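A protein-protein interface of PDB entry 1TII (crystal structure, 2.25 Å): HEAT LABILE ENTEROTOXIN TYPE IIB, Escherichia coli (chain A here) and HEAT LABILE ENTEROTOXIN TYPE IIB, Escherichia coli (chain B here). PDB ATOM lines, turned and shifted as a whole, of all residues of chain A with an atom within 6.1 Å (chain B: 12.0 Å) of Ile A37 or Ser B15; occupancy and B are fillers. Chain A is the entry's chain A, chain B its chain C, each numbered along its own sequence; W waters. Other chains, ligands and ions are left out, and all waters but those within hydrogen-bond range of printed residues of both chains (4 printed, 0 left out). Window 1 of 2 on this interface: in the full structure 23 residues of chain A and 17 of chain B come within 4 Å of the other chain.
Of chain B, only Asn B12 (3.4 Å) comes within 4 Å of Asn A36.
Ile A37 touches just these residues of chain B: Asn B12, Ser B15 and Gln B16.
No residue of chain B comes within 4 Å of Asn A38.
Leu A39 touches none of the printed residues of chain B.
No residue of chain B comes within 4 Å of Asp A55.
Gly A115 touches one residue of chain B.
Of the printed residues of chain B, Ile A162 touches Leu B14 (3.9 Å), Ser B15 (3.5 Å) and Asp B18 (3.7 Å).
Printed residues of chain A within 4 Å of Leu B14: Ile A162 (3.9 Å).
Ser B15 touches just these residues of chain A: Ile A37 and Ile A162.
Of the printed residues of chain A, Leu B19 touches Pro A34 (3.8 Å), Leu A114 (3.4 Å) and Gly A115 (3.7 Å).
The nearest printed residue of chain B that does not touch Ile A37 is Thr B11 (4.02 Å).
The nearest printed residue of chain A that does not touch Leu B19 is Ile A37 (4.02 Å).
The side-chain amide oxygen of Asn A36 lies close to the side-chain carboxylate of Asp A55.
O of Asn A36 is in hydrogen-bond range of N of Gly A56 (3.2 Å).
The backbone carbonyl oxygen of Gly A56 lies within hydrogen-bond range of the backbone NH of Gly A115, 2.7 Å away.
The backbone carbonyl oxygen of Thr B11 sits at hydrogen-bond distance from the side-chain hydroxyl of Ser B15 (3.1 Å).
NE2 of Gln B16 sits at hydrogen-bond distance from OD1 of Asn B12 (3.4 Å).
The side-chain amide nitrogen of Gln B16 sits at hydrogen-bond distance from the backbone carbonyl oxygen of Pro A34 (2.9 Å).
The backbone NH (N) of Ile A37 lies within hydrogen-bond range of the side-chain amide oxygen (OD1) of Asn B12 (2.8 Å).
Of the 20 printed residues of chain B, 6 touch a printed residue of chain A.
Printed residues of chain B that touch a printed residue of chain A: Asn B12, Leu B14, Ser B15, Gln B16, Asp B18 and Leu B19.
Along chain B the printed residues that touch a printed residue of chain A span positions 12 to 19.
Of the 12 printed residues of chain A, 6 touch a printed residue of chain B.
Hydrophobic or aromatic side chains of chain A that line the printed part of chain B: Pro A34, Ile A37, Leu A114 and Ile A162.
Along chain A the printed residues that touch a printed residue of chain B span positions 34 to 162.
Among the printed residues, 12 pairs touch across the chains.
Among the printed residues, no Asp or Glu carboxylate lies within 4 Å of a Lys or Arg side-chain nitrogen of the other chain.
Among the printed residues, merely in contact across the chains: Pro A34 with Leu B19 (3.8 Å), Asn A36 with Asn B12 (3.4 Å), Ile A37 with Ser B15 (3.5 Å), Ile A37 with Gln B16 (3.7 Å), Leu A114 with Asp B18 (3.6 Å), Leu A114 with Leu B19 (3.4 Å), Gly A115 with Leu B19 (3.7 Å), Ile A162 with Leu B14 (3.9 Å), Ile A162 with Ser B15 (3.5 Å) and Ile A162 with Asp B18 (3.7 Å).
Water W2 lies within hydrogen-bond range of O of Ile A162 (2.7 Å), OG of Ser B15 (2.8 Å), OH of Tyr A57 (2.8 Å) and N of Leu A39 (3.1 Å).
Water W3 bridges the backbone carbonyl oxygen of Gly A115 (2.9 Å) and the side-chain amino group of Lys B23 (2.9 Å).
Water W1 lies within hydrogen-bond range of OG1 of Thr B11 (2.9 Å), ND2 of Asn A38 (3.4 Å) and SG of Cys B7 (3.6 Å).
Water W4 lies within hydrogen-bond range of the backbone carbonyl oxygen (O) of Ala B8, the side-chain amide nitrogen (ND2) of Asn A38, the side-chain amide nitrogen (ND2) of Asn A36 and the backbone carbonyl oxygen (O) of Ile A37.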
ATOM      1  N   PRO A  34      25.004 -22.926 -31.768  1.00  0.00           N
ATOM      2  CA  PRO A  34      24.568 -24.319 -31.596  1.00  0.00           C
ATOM      3  C   PRO A  34      23.049 -24.283 -31.800  1.00  0.00           C
ATOM      4  O   PRO A  34      22.408 -23.283 -31.461  1.00  0.00           O
ATOM      5  CB  PRO A  34      24.903 -24.599 -30.132  1.00  0.00           C
ATOM      6  CG  PRO A  34      26.047 -23.649 -29.853  1.00  0.00           C
ATOM      7  CD  PRO A  34      25.623 -22.404 -30.537  1.00  0.00           C
ATOM      8  N   ILE A  35      22.448 -25.330 -32.346  1.00  0.00           N
ATOM      9  CA  ILE A  35      21.001 -25.276 -32.546  1.00  0.00           C
ATOM     10  C   ILE A  35      20.259 -25.404 -31.212  1.00  0.00           C
ATOM     11  O   ILE A  35      19.142 -24.914 -31.063  1.00  0.00           O
ATOM     12  CB  ILE A  35      20.513 -26.301 -33.592  1.00  0.00           C
ATOM     13  CG1 ILE A  35      20.917 -27.723 -33.194  1.00  0.00           C
ATOM     14  CG2 ILE A  35      21.087 -25.942 -34.960  1.00  0.00           C
ATOM     15  CD1 ILE A  35      20.911 -28.722 -34.350  1.00  0.00           C
ATOM     16  N   ASN A  36      20.902 -26.033 -30.235  1.00  0.00           N
ATOM     17  CA  ASN A  36      20.335 -26.194 -28.906  1.00  0.00           C
ATOM     18  C   ASN A  36      21.456 -26.192 -27.871  1.00  0.00           C
ATOM     19  O   ASN A  36      22.462 -26.863 -28.046  1.00  0.00           O
ATOM     20  CB  ASN A  36      19.528 -27.485 -28.805  1.00  0.00           C
ATOM     21  CG  ASN A  36      19.068 -27.780 -27.380  1.00  0.00           C
ATOM     22  OD1 ASN A  36      19.618 -28.669 -26.718  1.00  0.00           O
ATOM     23  ND2 ASN A  36      18.057 -27.050 -26.907  1.00  0.00           N
ATOM     24  N   ILE A  37      21.297 -25.383 -26.829  1.00  0.00           N
ATOM     25  CA  ILE A  37      22.275 -25.286 -25.758  1.00  0.00           C
ATOM     26  C   ILE A  37      21.610 -25.747 -24.452  1.00  0.00           C
ATOM     27  O   ILE A  37      20.566 -25.231 -24.083  1.00  0.00           O
ATOM     28  CB  ILE A  37      22.762 -23.837 -25.567  1.00  0.00           C
ATOM     29  CG1 ILE A  37      23.206 -23.230 -26.894  1.00  0.00           C
ATOM     30  CG2 ILE A  37      23.903 -23.805 -24.578  1.00  0.00           C
ATOM     31  CD1 ILE A  37      24.073 -21.984 -26.742  1.00  0.00           C
ATOM     32  N   ASN A  38      22.191 -26.739 -23.784  1.00  0.00           N
ATOM     33  CA  ASN A  38      21.668 -27.241 -22.517  1.00  0.00           C
ATOM     34  C   ASN A  38      22.812 -27.911 -21.748  1.00  0.00           C
ATOM     35  O   ASN A  38      23.259 -29.005 -22.119  1.00  0.00           O
ATOM     36  CB  ASN A  38      20.530 -28.233 -22.754  1.00  0.00           C
ATOM     37  CG  ASN A  38      19.891 -28.708 -21.463  1.00  0.00           C
ATOM     38  OD1 ASN A  38      20.550 -29.325 -20.604  1.00  0.00           O
ATOM     39  ND2 ASN A  38      18.611 -28.410 -21.307  1.00  0.00           N
ATOM     40  N   LEU A  39      23.274 -27.272 -20.670  1.00  0.00           N
ATOM     41  CA  LEU A  39      24.387 -27.814 -19.894  1.00  0.00           C
ATOM     42  C   LEU A  39      24.165 -29.203 -19.347  1.00  0.00           C
ATOM     43  O   LEU A  39      25.055 -30.036 -19.438  1.00  0.00           O
ATOM     44  CB  LEU A  39      24.798 -26.864 -18.758  1.00  0.00           C
ATOM     45  CG  LEU A  39      25.977 -27.257 -17.855  1.00  0.00           C
ATOM     46  CD1 LEU A  39      27.194 -27.614 -18.709  1.00  0.00           C
ATOM     47  CD2 LEU A  39      26.316 -26.117 -16.909  1.00  0.00           C
ATOM     48  N   ASP A  55      25.212 -30.560 -27.477  1.00  0.00           N
ATOM     49  CA  ASP A  55      24.315 -29.614 -26.829  1.00  0.00           C
ATOM     50  C   ASP A  55      24.872 -28.247 -26.525  1.00  0.00           C
ATOM     51  O   ASP A  55      24.741 -27.762 -25.401  1.00  0.00           O
ATOM     52  CB  ASP A  55      23.723 -30.212 -25.556  1.00  0.00           C
ATOM     53  CG  ASP A  55      22.879 -31.424 -25.836  1.00  0.00           C
ATOM     54  OD1 ASP A  55      21.774 -31.259 -26.374  1.00  0.00           O
ATOM     55  OD2 ASP A  55      23.328 -32.546 -25.532  1.00  0.00           O
ATOM     56  N   GLY A  56      25.505 -27.646 -27.524  1.00  0.00           N
ATOM     57  CA  GLY A  56      26.036 -26.306 -27.398  1.00  0.00           C
ATOM     58  C   GLY A  56      27.249 -26.024 -26.557  1.00  0.00           C
ATOM     59  O   GLY A  56      27.637 -24.861 -26.421  1.00  0.00           O
ATOM     60  N   TYR A  57      27.881 -27.050 -26.022  1.00  0.00           N
ATOM     61  CA  TYR A  57      29.056 -26.839 -25.190  1.00  0.00           C
ATOM     62  C   TYR A  57      30.205 -27.726 -25.679  1.00  0.00           C
ATOM     63  O   TYR A  57      29.988 -28.793 -26.241  1.00  0.00           O
ATOM     64  CB  TYR A  57      28.752 -27.208 -23.717  1.00  0.00           C
ATOM     65  CG  TYR A  57      27.854 -26.259 -22.915  1.00  0.00           C
ATOM     66  CD1 TYR A  57      26.455 -26.325 -22.988  1.00  0.00           C
ATOM     67  CD2 TYR A  57      28.414 -25.317 -22.056  1.00  0.00           C
ATOM     68  CE1 TYR A  57      25.653 -25.461 -22.221  1.00  0.00           C
ATOM     69  CE2 TYR A  57      27.624 -24.471 -21.296  1.00  0.00           C
ATOM     70  CZ  TYR A  57      26.253 -24.545 -21.389  1.00  0.00           C
ATOM     71  OH  TYR A  57      25.539 -23.655 -20.651  1.00  0.00           O
ATOM     72  N   LEU A 114      30.751 -22.629 -23.225  1.00  0.00           N
ATOM     73  CA  LEU A 114      29.504 -22.242 -23.866  1.00  0.00           C
ATOM     74  C   LEU A 114      29.718 -21.828 -25.317  1.00  0.00           C
ATOM     75  O   LEU A 114      30.432 -20.876 -25.594  1.00  0.00           O
ATOM     76  CB  LEU A 114      28.836 -21.105 -23.076  1.00  0.00           C
ATOM     77  CG  LEU A 114      27.585 -20.391 -23.634  1.00  0.00           C
ATOM     78  CD1 LEU A 114      26.467 -21.353 -23.932  1.00  0.00           C
ATOM     79  CD2 LEU A 114      27.126 -19.322 -22.658  1.00  0.00           C
ATOM     80  N   GLY A 115      29.060 -22.530 -26.232  1.00  0.00           N
ATOM     81  CA  GLY A 115      29.185 -22.219 -27.647  1.00  0.00           C
ATOM     82  C   GLY A 115      30.535 -22.530 -28.294  1.00  0.00           C
ATOM     83  O   GLY A 115      30.736 -22.225 -29.466  1.00  0.00           O
ATOM     84  N   ILE A 162      21.316 -21.317 -16.092  1.00  0.00           N
ATOM     85  CA  ILE A 162      21.301 -22.099 -17.339  1.00  0.00           C
ATOM     86  C   ILE A 162      21.668 -23.578 -17.183  1.00  0.00           C
ATOM     87  O   ILE A 162      22.007 -24.248 -18.151  1.00  0.00           O
ATOM     88  CB  ILE A 162      22.185 -21.437 -18.469  1.00  0.00           C
ATOM     89  CG1 ILE A 162      23.623 -21.169 -17.986  1.00  0.00           C
ATOM     90  CG2 ILE A 162      21.535 -20.150 -18.942  1.00  0.00           C
ATOM     91  CD1 ILE A 162      24.596 -20.896 -19.084  1.00  0.00           C
ATOM     92  N   THR B   5       6.397 -20.571 -22.672  1.00  0.00           N
ATOM     93  CA  THR B   5       7.665 -21.252 -23.096  1.00  0.00           C
ATOM     94  C   THR B   5       7.914 -22.465 -22.201  1.00  0.00           C
ATOM     95  O   THR B   5       7.445 -22.494 -21.055  1.00  0.00           O
ATOM     96  CB  THR B   5       8.867 -20.306 -22.927  1.00  0.00           C
ATOM     97  OG1 THR B   5       8.534 -19.303 -21.956  1.00  0.00           O
ATOM     98  CG2 THR B   5       9.246 -19.651 -24.256  1.00  0.00           C
ATOM     99  N   THR B   6       8.607 -23.473 -22.726  1.00  0.00           N
ATOM    100  CA  THR B   6       8.915 -24.648 -21.922  1.00  0.00           C
ATOM    101  C   THR B   6      10.195 -24.386 -21.141  1.00  0.00           C
ATOM    102  O   THR B   6      10.892 -23.380 -21.357  1.00  0.00           O
ATOM    103  CB  THR B   6       9.137 -25.894 -22.772  1.00  0.00           C
ATOM    104  OG1 THR B   6      10.301 -25.716 -23.587  1.00  0.00           O
ATOM    105  CG2 THR B   6       7.941 -26.152 -23.647  1.00  0.00           C
ATOM    106  N   CYS B   7      10.496 -25.285 -20.223  1.00  0.00           N
ATOM    107  CA  CYS B   7      11.694 -25.163 -19.432  1.00  0.00           C
ATOM    108  C   CYS B   7      12.887 -25.223 -20.404  1.00  0.00           C
ATOM    109  O   CYS B   7      13.742 -24.340 -20.403  1.00  0.00           O
ATOM    110  CB  CYS B   7      11.729 -26.295 -18.425  1.00  0.00           C
ATOM    111  SG  CYS B   7      13.178 -26.301 -17.362  1.00  0.00           S
ATOM    112  N   ALA B   8      12.842 -26.176 -21.329  1.00  0.00           N
ATOM    113  CA  ALA B   8      13.897 -26.365 -22.329  1.00  0.00           C
ATOM    114  C   ALA B   8      14.167 -25.129 -23.157  1.00  0.00           C
ATOM    115  O   ALA B   8      15.273 -24.600 -23.156  1.00  0.00           O
ATOM    116  CB  ALA B   8      13.548 -27.498 -23.231  1.00  0.00           C
ATOM    117  N   SER B   9      13.120 -24.636 -23.809  1.00  0.00           N
ATOM    118  CA  SER B   9      13.212 -23.460 -24.653  1.00  0.00           C
ATOM    119  C   SER B   9      13.748 -22.264 -23.930  1.00  0.00           C
ATOM    120  O   SER B   9      14.573 -21.516 -24.455  1.00  0.00           O
ATOM    121  CB  SER B   9      11.848 -23.117 -25.231  1.00  0.00           C
ATOM    122  OG  SER B   9      11.303 -24.246 -25.880  1.00  0.00           O
ATOM    123  N   LEU B  10      13.287 -22.061 -22.717  1.00  0.00           N
ATOM    124  CA  LEU B  10      13.766 -20.911 -22.000  1.00  0.00           C
ATOM    125  C   LEU B  10      15.238 -21.109 -21.642  1.00  0.00           C
ATOM    126  O   LEU B  10      15.988 -20.142 -21.580  1.00  0.00           O
ATOM    127  CB  LEU B  10      12.908 -20.641 -20.770  1.00  0.00           C
ATOM    128  CG  LEU B  10      13.144 -19.270 -20.147  1.00  0.00           C
ATOM    129  CD1 LEU B  10      12.975 -18.178 -21.192  1.00  0.00           C
ATOM    130  CD2 LEU B  10      12.192 -19.066 -18.999  1.00  0.00           C
ATOM    131  N   THR B  11      15.655 -22.344 -21.387  1.00  0.00           N
ATOM    132  CA  THR B  11      17.056 -22.586 -21.066  1.00  0.00           C
ATOM    133  C   THR B  11      17.885 -22.266 -22.302  1.00  0.00           C
ATOM    134  O   THR B  11      18.829 -21.504 -22.226  1.00  0.00           O
ATOM    135  CB  THR B  11      17.334 -24.045 -20.706  1.00  0.00           C
ATOM    136  OG1 THR B  11      16.706 -24.366 -19.464  1.00  0.00           O
ATOM    137  CG2 THR B  11      18.823 -24.274 -20.587  1.00  0.00           C
ATOM    138  N   ASN B  12      17.514 -22.851 -23.436  1.00  0.00           N
ATOM    139  CA  ASN B  12      18.226 -22.626 -24.687  1.00  0.00           C
ATOM    140  C   ASN B  12      18.309 -21.135 -24.943  1.00  0.00           C
ATOM    141  O   ASN B  12      19.394 -20.585 -25.115  1.00  0.00           O
ATOM    142  CB  ASN B  12      17.501 -23.311 -25.845  1.00  0.00           C
ATOM    143  CG  ASN B  12      18.202 -23.103 -27.176  1.00  0.00           C
ATOM    144  OD1 ASN B  12      19.387 -23.395 -27.317  1.00  0.00           O
ATOM    145  ND2 ASN B  12      17.480 -22.593 -28.152  1.00  0.00           N
ATOM    146  N   LYS B  13      17.156 -20.477 -24.880  1.00  0.00           N
ATOM    147  CA  LYS B  13      17.032 -19.043 -25.101  1.00  0.00           C
ATOM    148  C   LYS B  13      17.959 -18.207 -24.220  1.00  0.00           C
ATOM    149  O   LYS B  13      18.621 -17.286 -24.690  1.00  0.00           O
ATOM    150  CB  LYS B  13      15.566 -18.638 -24.906  1.00  0.00           C
ATOM    151  CG  LYS B  13      15.254 -17.165 -25.126  1.00  0.00           C
ATOM    152  CD  LYS B  13      13.771 -16.974 -25.503  1.00  0.00           C
ATOM    153  CE  LYS B  13      13.411 -15.487 -25.673  1.00  0.00           C
ATOM    154  NZ  LYS B  13      12.027 -15.260 -26.208  1.00  0.00           N
ATOM    155  N   LEU B  14      17.998 -18.520 -22.938  1.00  0.00           N
ATOM    156  CA  LEU B  14      18.850 -17.794 -22.027  1.00  0.00           C
ATOM    157  C   LEU B  14      20.313 -18.074 -22.386  1.00  0.00           C
ATOM    158  O   LEU B  14      21.159 -17.166 -22.373  1.00  0.00           O
ATOM    159  CB  LEU B  14      18.544 -18.218 -20.590  1.00  0.00           C
ATOM    160  CG  LEU B  14      17.126 -17.844 -20.148  1.00  0.00           C
ATOM    161  CD1 LEU B  14      16.743 -18.484 -18.828  1.00  0.00           C
ATOM    162  CD2 LEU B  14      17.055 -16.368 -20.040  1.00  0.00           C
ATOM    163  N   SER B  15      20.599 -19.327 -22.724  1.00  0.00           N
ATOM    164  CA  SER B  15      21.940 -19.739 -23.080  1.00  0.00           C
ATOM    165  C   SER B  15      22.432 -19.027 -24.336  1.00  0.00           C
ATOM    166  O   SER B  15      23.553 -18.553 -24.365  1.00  0.00           O
ATOM    167  CB  SER B  15      22.000 -21.250 -23.237  1.00  0.00           C
ATOM    168  OG  SER B  15      21.906 -21.852 -21.962  1.00  0.00           O
ATOM    169  N   GLN B  16      21.575 -18.896 -25.340  1.00  0.00           N
ATOM    170  CA  GLN B  16      21.954 -18.215 -26.566  1.00  0.00           C
ATOM    171  C   GLN B  16      22.294 -16.760 -26.274  1.00  0.00           C
ATOM    172  O   GLN B  16      23.238 -16.215 -26.828  1.00  0.00           O
ATOM    173  CB  GLN B  16      20.839 -18.294 -27.607  1.00  0.00           C
ATOM    174  CG  GLN B  16      20.482 -19.701 -28.081  1.00  0.00           C
ATOM    175  CD  GLN B  16      21.483 -20.314 -29.051  1.00  0.00           C
ATOM    176  OE1 GLN B  16      22.486 -19.704 -29.417  1.00  0.00           O
ATOM    177  NE2 GLN B  16      21.217 -21.543 -29.453  1.00  0.00           N
ATOM    178  N   HIS B  17      21.585 -16.154 -25.332  1.00  0.00           N
ATOM    179  CA  HIS B  17      21.823 -14.762 -24.999  1.00  0.00           C
ATOM    180  C   HIS B  17      23.159 -14.617 -24.322  1.00  0.00           C
ATOM    181  O   HIS B  17      23.865 -13.643 -24.534  1.00  0.00           O
ATOM    182  CB  HIS B  17      20.704 -14.212 -24.104  1.00  0.00           C
ATOM    183  CG  HIS B  17      20.834 -12.749 -23.813  1.00  0.00           C
ATOM    184  ND1 HIS B  17      21.239 -12.269 -22.583  1.00  0.00           N
ATOM    185  CD2 HIS B  17      20.691 -11.667 -24.615  1.00  0.00           C
ATOM    186  CE1 HIS B  17      21.347 -10.953 -22.645  1.00  0.00           C
ATOM    187  NE2 HIS B  17      21.022 -10.562 -23.865  1.00  0.00           N
ATOM    188  N   ASP B  18      23.488 -15.561 -23.462  1.00  0.00           N
ATOM    189  CA  ASP B  18      24.768 -15.520 -22.791  1.00  0.00           C
ATOM    190  C   ASP B  18      25.930 -15.627 -23.788  1.00  0.00           C
ATOM    191  O   ASP B  18      26.930 -14.942 -23.651  1.00  0.00           O
ATOM    192  CB  ASP B  18      24.861 -16.653 -21.787  1.00  0.00           C
ATOM    193  CG  ASP B  18      24.096 -16.372 -20.532  1.00  0.00           C
ATOM    194  OD1 ASP B  18      23.572 -15.241 -20.376  1.00  0.00           O
ATOM    195  OD2 ASP B  18      24.038 -17.292 -19.694  1.00  0.00           O
ATOM    196  N   LEU B  19      25.798 -16.516 -24.758  1.00  0.00           N
ATOM    197  CA  LEU B  19      26.815 -16.706 -25.782  1.00  0.00           C
ATOM    198  C   LEU B  19      27.004 -15.423 -26.586  1.00  0.00           C
ATOM    199  O   LEU B  19      28.105 -14.904 -26.673  1.00  0.00           O
ATOM    200  CB  LEU B  19      26.393 -17.844 -26.708  1.00  0.00           C
ATOM    201  CG  LEU B  19      27.346 -18.268 -27.821  1.00  0.00           C
ATOM    202  CD1 LEU B  19      28.772 -18.481 -27.289  1.00  0.00           C
ATOM    203  CD2 LEU B  19      26.796 -19.538 -28.411  1.00  0.00           C
ATOM    204  N   ALA B  20      25.919 -14.919 -27.157  1.00  0.00           N
ATOM    205  CA  ALA B  20      25.921 -13.699 -27.940  1.00  0.00           C
ATOM    206  C   ALA B  20      26.618 -12.601 -27.195  1.00  0.00           C
ATOM    207  O   ALA B  20      27.419 -11.878 -27.764  1.00  0.00           O
ATOM    208  CB  ALA B  20      24.506 -13.279 -28.255  1.00  0.00           C
ATOM    209  N   ASP B  21      26.349 -12.490 -25.902  1.00  0.00           N
ATOM    210  CA  ASP B  21      26.996 -11.457 -25.101  1.00  0.00           C
ATOM    211  C   ASP B  21      28.494 -11.656 -24.961  1.00  0.00           C
ATOM    212  O   ASP B  21      29.236 -10.683 -24.885  1.00  0.00           O
ATOM    213  CB  ASP B  21      26.379 -11.379 -23.712  1.00  0.00           C
ATOM    214  CG  ASP B  21      25.064 -10.602 -23.691  1.00  0.00           C
ATOM    215  OD1 ASP B  21      24.552 -10.175 -24.759  1.00  0.00           O
ATOM    216  OD2 ASP B  21      24.537 -10.426 -22.577  1.00  0.00           O
ATOM    217  N   PHE B  22      28.931 -12.911 -24.851  1.00  0.00           N
ATOM    218  CA  PHE B  22      30.352 -13.240 -24.717  1.00  0.00           C
ATOM    219  C   PHE B  22      31.052 -12.873 -26.024  1.00  0.00           C
ATOM    220  O   PHE B  22      32.079 -12.188 -26.021  1.00  0.00           O
ATOM    221  CB  PHE B  22      30.551 -14.736 -24.406  1.00  0.00           C
ATOM    222  CG  PHE B  22      32.002 -15.154 -24.351  1.00  0.00           C
ATOM    223  CD1 PHE B  22      32.841 -14.689 -23.325  1.00  0.00           C
ATOM    224  CD2 PHE B  22      32.553 -15.943 -25.366  1.00  0.00           C
ATOM    225  CE1 PHE B  22      34.208 -14.997 -23.314  1.00  0.00           C
ATOM    226  CE2 PHE B  22      33.917 -16.254 -25.360  1.00  0.00           C
ATOM    227  CZ  PHE B  22      34.746 -15.775 -24.329  1.00  0.00           C
ATOM    228  N   LYS B  23      30.467 -13.301 -27.135  1.00  0.00           N
ATOM    229  CA  LYS B  23      31.012 -12.987 -28.433  1.00  0.00           C
ATOM    230  C   LYS B  23      31.139 -11.479 -28.627  1.00  0.00           C
ATOM    231  O   LYS B  23      32.185 -11.012 -29.101  1.00  0.00           O
ATOM    232  CB  LYS B  23      30.180 -13.618 -29.522  1.00  0.00           C
ATOM    233  CG  LYS B  23      30.367 -15.102 -29.578  1.00  0.00           C
ATOM    234  CD  LYS B  23      29.627 -15.673 -30.758  1.00  0.00           C
ATOM    235  CE  LYS B  23      29.782 -17.174 -30.794  1.00  0.00           C
ATOM    236  NZ  LYS B  23      28.913 -17.808 -31.825  1.00  0.00           N
ATOM    237  N   LYS B  24      30.124 -10.708 -28.217  1.00  0.00           N
ATOM    238  CA  LYS B  24      30.197  -9.245 -28.332  1.00  0.00           C
ATOM    239  C   LYS B  24      31.319  -8.717 -27.463  1.00  0.00           C
ATOM    240  O   LYS B  24      32.006  -7.782 -27.830  1.00  0.00           O
ATOM    241  CB  LYS B  24      28.912  -8.553 -27.880  1.00  0.00           C
ATOM    242  CG  LYS B  24      27.689  -8.791 -28.721  1.00  0.00           C
ATOM    243  CD  LYS B  24      26.642  -7.736 -28.374  1.00  0.00           C
ATOM    244  CE  LYS B  24      25.228  -8.158 -28.767  1.00  0.00           C
ATOM    245  NZ  LYS B  24      24.532  -8.987 -27.718  1.00  0.00           N
HETATM  246  O   HOH W   1      16.144 -27.228 -19.256  1.00  0.00           O
HETATM  247  O   HOH W   2      22.794 -24.209 -20.784  1.00  0.00           O
HETATM  248  O   HOH W   3      29.127 -20.685 -31.247  1.00  0.00           O
HETATM  249  O   HOH W   4      17.497 -26.568 -23.694  1.00  0.00           O
